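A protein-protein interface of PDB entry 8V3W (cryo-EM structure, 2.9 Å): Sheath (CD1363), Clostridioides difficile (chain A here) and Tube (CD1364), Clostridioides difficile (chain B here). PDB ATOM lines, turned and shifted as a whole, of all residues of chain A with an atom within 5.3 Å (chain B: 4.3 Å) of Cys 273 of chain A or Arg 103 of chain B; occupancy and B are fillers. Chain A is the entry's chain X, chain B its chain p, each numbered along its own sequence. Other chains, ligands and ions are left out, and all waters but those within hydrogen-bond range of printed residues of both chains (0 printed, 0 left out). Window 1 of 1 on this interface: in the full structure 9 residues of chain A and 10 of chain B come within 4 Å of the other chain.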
ATOM      1  N   TYR A 269      35.476  -6.643  25.368  1.00  0.00           N
ATOM      2  CA  TYR A 269      34.033  -6.426  25.325  1.00  0.00           C
ATOM      3  C   TYR A 269      33.264  -7.735  25.475  1.00  0.00           C
ATOM      4  O   TYR A 269      32.212  -7.781  26.131  1.00  0.00           O
ATOM      5  CB  TYR A 269      33.669  -5.719  24.020  1.00  0.00           C
ATOM      6  CG  TYR A 269      32.225  -5.302  23.914  1.00  0.00           C
ATOM      7  CD1 TYR A 269      31.663  -4.432  24.832  1.00  0.00           C
ATOM      8  CD2 TYR A 269      31.428  -5.771  22.886  1.00  0.00           C
ATOM      9  CE1 TYR A 269      30.347  -4.051  24.733  1.00  0.00           C
ATOM     10  CE2 TYR A 269      30.113  -5.396  22.779  1.00  0.00           C
ATOM     11  CZ  TYR A 269      29.576  -4.536  23.704  1.00  0.00           C
ATOM     12  OH  TYR A 269      28.259  -4.161  23.595  1.00  0.00           O
ATOM     13  N   ASP A 270      33.775  -8.812  24.876  1.00  0.00           N
ATOM     14  CA  ASP A 270      33.108 -10.106  24.970  1.00  0.00           C
ATOM     15  C   ASP A 270      33.018 -10.582  26.413  1.00  0.00           C
ATOM     16  O   ASP A 270      31.993 -11.131  26.836  1.00  0.00           O
ATOM     17  CB  ASP A 270      33.849 -11.131  24.115  1.00  0.00           C
ATOM     18  CG  ASP A 270      33.826 -10.787  22.643  1.00  0.00           C
ATOM     19  OD1 ASP A 270      33.046  -9.895  22.254  1.00  0.00           O
ATOM     20  OD2 ASP A 270      34.588 -11.406  21.874  1.00  0.00           O
ATOM     21  N   ASN A 271      34.088 -10.386  27.183  1.00  0.00           N
ATOM     22  CA  ASN A 271      34.069 -10.782  28.583  1.00  0.00           C
ATOM     23  C   ASN A 271      33.111  -9.920  29.392  1.00  0.00           C
ATOM     24  O   ASN A 271      32.498 -10.408  30.350  1.00  0.00           O
ATOM     25  CB  ASN A 271      35.486 -10.727  29.147  1.00  0.00           C
ATOM     26  CG  ASN A 271      36.466 -11.542  28.322  1.00  0.00           C
ATOM     27  OD1 ASN A 271      37.514 -11.050  27.916  1.00  0.00           O
ATOM     28  ND2 ASN A 271      36.114 -12.791  28.054  1.00  0.00           N
ATOM     29  N   LYS A 272      32.951  -8.649  29.018  1.00  0.00           N
ATOM     30  CA  LYS A 272      31.930  -7.825  29.654  1.00  0.00           C
ATOM     31  C   LYS A 272      30.537  -8.379  29.387  1.00  0.00           C
ATOM     32  O   LYS A 272      29.693  -8.422  30.290  1.00  0.00           O
ATOM     33  CB  LYS A 272      32.035  -6.383  29.165  1.00  0.00           C
ATOM     34  CG  LYS A 272      33.372  -5.735  29.434  1.00  0.00           C
ATOM     35  CD  LYS A 272      33.380  -4.279  29.011  1.00  0.00           C
ATOM     36  CE  LYS A 272      34.785  -3.706  29.082  1.00  0.00           C
ATOM     37  NZ  LYS A 272      34.838  -2.290  28.640  1.00  0.00           N
ATOM     38  N   CYS A 273      30.279  -8.810  28.151  1.00  0.00           N
ATOM     39  CA  CYS A 273      28.980  -9.403  27.843  1.00  0.00           C
ATOM     40  C   CYS A 273      28.757 -10.689  28.631  1.00  0.00           C
ATOM     41  O   CYS A 273      27.654 -10.942  29.132  1.00  0.00           O
ATOM     42  CB  CYS A 273      28.865  -9.658  26.343  1.00  0.00           C
ATOM     43  SG  CYS A 273      28.859  -8.152  25.345  1.00  0.00           S
ATOM     44  N   LEU A 274      29.799 -11.512  28.756  1.00  0.00           N
ATOM     45  CA  LEU A 274      29.687 -12.734  29.547  1.00  0.00           C
ATOM     46  C   LEU A 274      29.370 -12.424  31.009  1.00  0.00           C
ATOM     47  O   LEU A 274      28.530 -13.093  31.629  1.00  0.00           O
ATOM     48  CB  LEU A 274      30.976 -13.545  29.436  1.00  0.00           C
ATOM     49  CG  LEU A 274      31.186 -14.298  28.121  1.00  0.00           C
ATOM     50  CD1 LEU A 274      32.599 -14.818  28.020  1.00  0.00           C
ATOM     51  CD2 LEU A 274      30.194 -15.441  27.995  1.00  0.00           C
ATOM     52  N   LEU A 275      30.035 -11.415  31.576  1.00  0.00           N
ATOM     53  CA  LEU A 275      29.763 -11.024  32.956  1.00  0.00           C
ATOM     54  C   LEU A 275      28.331 -10.523  33.118  1.00  0.00           C
ATOM     55  O   LEU A 275      27.662 -10.828  34.116  1.00  0.00           O
ATOM     56  CB  LEU A 275      30.766  -9.958  33.395  1.00  0.00           C
ATOM     57  CG  LEU A 275      30.520  -9.231  34.714  1.00  0.00           C
ATOM     58  CD1 LEU A 275      30.520 -10.207  35.869  1.00  0.00           C
ATOM     59  CD2 LEU A 275      31.563  -8.151  34.926  1.00  0.00           C
ATOM     60  N   ILE A 276      27.845  -9.747  32.146  1.00  0.00           N
ATOM     61  CA  ILE A 276      26.459  -9.292  32.184  1.00  0.00           C
ATOM     62  C   ILE A 276      25.512 -10.481  32.197  1.00  0.00           C
ATOM     63  O   ILE A 276      24.531 -10.506  32.951  1.00  0.00           O
ATOM     64  CB  ILE A 276      26.167  -8.358  30.996  1.00  0.00           C
ATOM     65  CG1 ILE A 276      26.917  -7.040  31.150  1.00  0.00           C
ATOM     66  CG2 ILE A 276      24.685  -8.097  30.880  1.00  0.00           C
ATOM     67  CD1 ILE A 276      26.859  -6.182  29.922  1.00  0.00           C
ATOM     68  N   VAL A 277      25.787 -11.484  31.362  1.00  0.00           N
ATOM     69  CA  VAL A 277      24.924 -12.662  31.302  1.00  0.00           C
ATOM     70  C   VAL A 277      24.916 -13.391  32.640  1.00  0.00           C
ATOM     71  O   VAL A 277      23.865 -13.846  33.111  1.00  0.00           O
ATOM     72  CB  VAL A 277      25.363 -13.582  30.150  1.00  0.00           C
ATOM     73  CG1 VAL A 277      24.648 -14.914  30.225  1.00  0.00           C
ATOM     74  CG2 VAL A 277      25.098 -12.914  28.819  1.00  0.00           C
ATOM     75  N   ALA A 278      26.086 -13.520  33.272  1.00  0.00           N
ATOM     76  CA  ALA A 278      26.153 -14.196  34.567  1.00  0.00           C
ATOM     77  C   ALA A 278      25.342 -13.462  35.632  1.00  0.00           C
ATOM     78  O   ALA A 278      24.586 -14.082  36.398  1.00  0.00           O
ATOM     79  CB  ALA A 278      27.608 -14.339  35.008  1.00  0.00           C
ATOM     80  N   GLU A 326      32.004   0.021  22.568  1.00  0.00           N
ATOM     81  CA  GLU A 326      33.010  -1.031  22.538  1.00  0.00           C
ATOM     82  C   GLU A 326      34.433  -0.502  22.663  1.00  0.00           C
ATOM     83  O   GLU A 326      35.383  -1.255  22.435  1.00  0.00           O
ATOM     84  CB  GLU A 326      32.876  -1.853  21.255  1.00  0.00           C
ATOM     85  CG  GLU A 326      31.565  -2.603  21.138  1.00  0.00           C
ATOM     86  CD  GLU A 326      31.448  -3.369  19.836  1.00  0.00           C
ATOM     87  OE1 GLU A 326      32.471  -3.912  19.372  1.00  0.00           O
ATOM     88  OE2 GLU A 326      30.333  -3.433  19.280  1.00  0.00           O
ATOM     89  N   ILE B  90      25.561 -17.829  23.355  1.00  0.00           N
ATOM     90  CA  ILE B  90      25.680 -16.441  22.930  1.00  0.00           C
ATOM     91  C   ILE B  90      26.124 -16.438  21.477  1.00  0.00           C
ATOM     92  O   ILE B  90      27.155 -17.028  21.137  1.00  0.00           O
ATOM     93  CB  ILE B  90      26.671 -15.658  23.804  1.00  0.00           C
ATOM     94  CG1 ILE B  90      26.220 -15.672  25.263  1.00  0.00           C
ATOM     95  CG2 ILE B  90      26.817 -14.233  23.299  1.00  0.00           C
ATOM     96  CD1 ILE B  90      26.976 -14.712  26.140  1.00  0.00           C
ATOM     97  N   SER B  91      25.352 -15.774  20.620  1.00  0.00           N
ATOM     98  CA  SER B  91      25.657 -15.669  19.201  1.00  0.00           C
ATOM     99  C   SER B  91      25.935 -14.216  18.855  1.00  0.00           C
ATOM    100  O   SER B  91      25.191 -13.323  19.267  1.00  0.00           O
ATOM    101  CB  SER B  91      24.508 -16.205  18.349  1.00  0.00           C
ATOM    102  OG  SER B  91      23.259 -15.855  18.913  1.00  0.00           O
ATOM    103  N   LYS B  92      27.007 -13.982  18.104  1.00  0.00           N
ATOM    104  CA  LYS B  92      27.425 -12.641  17.726  1.00  0.00           C
ATOM    105  C   LYS B  92      27.595 -12.562  16.219  1.00  0.00           C
ATOM    106  O   LYS B  92      28.078 -13.508  15.591  1.00  0.00           O
ATOM    107  CB  LYS B  92      28.734 -12.252  18.415  1.00  0.00           C
ATOM    108  CG  LYS B  92      29.152 -10.818  18.175  1.00  0.00           C
ATOM    109  CD  LYS B  92      30.576 -10.571  18.625  1.00  0.00           C
ATOM    110  CE  LYS B  92      31.547 -10.620  17.466  1.00  0.00           C
ATOM    111  NZ  LYS B  92      32.887 -10.110  17.869  1.00  0.00           N
ATOM    112  N   GLU B 102      25.126  -7.585  16.189  1.00  0.00           N
ATOM    113  CA  GLU B 102      23.914  -8.201  16.718  1.00  0.00           C
ATOM    114  C   GLU B 102      24.334  -9.347  17.624  1.00  0.00           C
ATOM    115  O   GLU B 102      24.967 -10.299  17.160  1.00  0.00           O
ATOM    116  CB  GLU B 102      23.014  -8.703  15.586  1.00  0.00           C
ATOM    117  CG  GLU B 102      21.547  -8.820  15.948  1.00  0.00           C
ATOM    118  CD  GLU B 102      20.645  -8.833  14.722  1.00  0.00           C
ATOM    119  OE1 GLU B 102      20.442  -9.916  14.137  1.00  0.00           O
ATOM    120  OE2 GLU B 102      20.143  -7.757  14.339  1.00  0.00           O
ATOM    121  N   ARG B 103      23.983  -9.265  18.908  1.00  0.00           N
ATOM    122  CA  ARG B 103      24.477 -10.198  19.917  1.00  0.00           C
ATOM    123  C   ARG B 103      23.326 -10.669  20.797  1.00  0.00           C
ATOM    124  O   ARG B 103      22.842  -9.920  21.646  1.00  0.00           O
ATOM    125  CB  ARG B 103      25.570  -9.546  20.762  1.00  0.00           C
ATOM    126  CG  ARG B 103      26.446 -10.528  21.499  1.00  0.00           C
ATOM    127  CD  ARG B 103      27.423  -9.820  22.413  1.00  0.00           C
ATOM    128  NE  ARG B 103      28.296  -8.910  21.684  1.00  0.00           N
ATOM    129  CZ  ARG B 103      29.609  -9.055  21.586  1.00  0.00           C
ATOM    130  NH1 ARG B 103      30.237 -10.069  22.158  1.00  0.00           N
ATOM    131  NH2 ARG B 103      30.312  -8.162  20.898  1.00  0.00           N
ATOM    132  N   ILE B 104      22.912 -11.921  20.630  1.00  0.00           N
ATOM    133  CA  ILE B 104      21.745 -12.458  21.317  1.00  0.00           C
ATOM    134  C   ILE B 104      22.169 -13.627  22.192  1.00  0.00           C
ATOM    135  O   ILE B 104      23.013 -14.436  21.797  1.00  0.00           O
ATOM    136  CB  ILE B 104      20.659 -12.894  20.314  1.00  0.00           C
ATOM    137  CG1 ILE B 104      20.428 -11.788  19.286  1.00  0.00           C
ATOM    138  CG2 ILE B 104      19.371 -13.235  21.035  1.00  0.00           C
ATOM    139  CD1 ILE B 104      19.783 -12.270  18.016  1.00  0.00           C
ATOM    140  N   PHE B 138      18.359  -9.623  24.557  1.00  0.00           N
ATOM    141  CA  PHE B 138      18.883  -8.780  23.490  1.00  0.00           C
ATOM    142  C   PHE B 138      20.082  -7.983  23.986  1.00  0.00           C
ATOM    143  O   PHE B 138      19.988  -7.271  24.989  1.00  0.00           O
ATOM    144  CB  PHE B 138      17.810  -7.817  22.980  1.00  0.00           C
ATOM    145  CG  PHE B 138      16.931  -8.391  21.913  1.00  0.00           C
ATOM    146  CD1 PHE B 138      17.431  -9.289  20.992  1.00  0.00           C
ATOM    147  CD2 PHE B 138      15.600  -8.025  21.830  1.00  0.00           C
ATOM    148  CE1 PHE B 138      16.618  -9.815  20.013  1.00  0.00           C
ATOM    149  CE2 PHE B 138      14.783  -8.545  20.853  1.00  0.00           C
ATOM    150  CZ  PHE B 138      15.292  -9.440  19.944  1.00  0.00           C
ATOM    151  N   LEU B 139      21.197  -8.096  23.275  1.00  0.00           N
ATOM    152  CA  LEU B 139      22.363  -7.248  23.473  1.00  0.00           C
ATOM    153  C   LEU B 139      22.789  -6.712  22.114  1.00  0.00           C
ATOM    154  O   LEU B 139      22.815  -7.458  21.133  1.00  0.00           O
ATOM    155  CB  LEU B 139      23.522  -8.026  24.107  1.00  0.00           C
ATOM    156  CG  LEU B 139      23.191  -9.071  25.171  1.00  0.00           C
ATOM    157  CD1 LEU B 139      24.422  -9.881  25.535  1.00  0.00           C
ATOM    158  CD2 LEU B 139      22.631  -8.399  26.402  1.00  0.00           C
ATOM    159  N   ASP B 140      23.112  -5.426  22.046  1.00  0.00           N
ATOM    160  CA  ASP B 140      23.625  -4.819  20.818  1.00  0.00           C
ATOM    161  C   ASP B 140      22.726  -5.122  19.620  1.00  0.00           C
ATOM    162  O   ASP B 140      23.077  -5.892  18.729  1.00  0.00           O
ATOM    163  CB  ASP B 140      25.056  -5.282  20.535  1.00  0.00           C
ATOM    164  CG  ASP B 140      25.960  -5.160  21.736  1.00  0.00           C
ATOM    165  OD1 ASP B 140      25.480  -4.730  22.804  1.00  0.00           O
ATOM    166  OD2 ASP B 140      27.153  -5.498  21.610  1.00  0.00           O
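OD2 of Asp 140 of chain B is in hydrogen-bond range of OH of Tyr 269 of chain A (2.6 Å).
The guanidinium group (NH1) of Arg 103 of chain B lies within salt-bridge range of the side-chain carboxylate (OD1) of Asp 270 of chain A (2.8 Å).
SG of Cys 273 of chain A sits close to NE of Arg 103 of chain B (3.8 Å).
The backbone carbonyl oxygen (O) of Tyr 269 of chain A is in hydrogen-bond range of the side-chain sulfur (SG) of Cys 273 of chain A (3.5 Å).
The backbone carbonyl oxygen (O) of Arg 103 of chain B sits at hydrogen-bond distance from the backbone NH (N) of Leu 139 of chain B.
The side-chain carboxylate (OD2) of Asp 140 of chain B is in salt-bridge range of the guanidinium group (NE) of Arg 103 of chain B (3.6 Å).
NH2 of Arg 103 of chain B touches CD2 of Tyr 269 of chain A (3.3 Å).
Leu 274 of chain A touches Ile 90 of chain B (CD2 to CD1, 3.8 Å).
Val 277 of chain A touches Ile 90 of chain B.
Cys 273 of chain A touches just one residue of chain B: Arg 103.
Of chain A, only Tyr 269 (3.3 Å), Asp 270 (2.8 Å) and Cys 273 (3.7 Å) come within 4 Å of Arg 103 of chain B.
Printed residues of chain A within 4 Å of Ile 90 of chain B: Leu 274 and Val 277.
Printed residues of chain B within 4 Å of Val 277 of chain A: Ile 90.
Printed residues of chain B within 4 Å of Tyr 269 of chain A: Arg 103 and Asp 140.
Printed residues of chain A within 4 Å of Asp 140 of chain B: Tyr 269.
Of the printed residues of chain B, Asp 270 of chain A touches Arg 103 (2.8 Å).
The nearest printed residue of chain B that does not touch Cys 273 of chain A is Leu 139 of chain B (4.5 Å).
Of the 11 printed residues of chain A, 5 touch a printed residue of chain B.
Printed residues of chain B that touch a printed residue of chain A: Ile 90, Arg 103 and Asp 140.
Hydrophobic or aromatic side chains of chain B within 4 Å of the printed part of chain A: Ile 90.
Along chain B the printed residues that touch a printed residue of chain A span positions 90 to 140.
Among the printed residues, 6 pairs touch across the chains.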
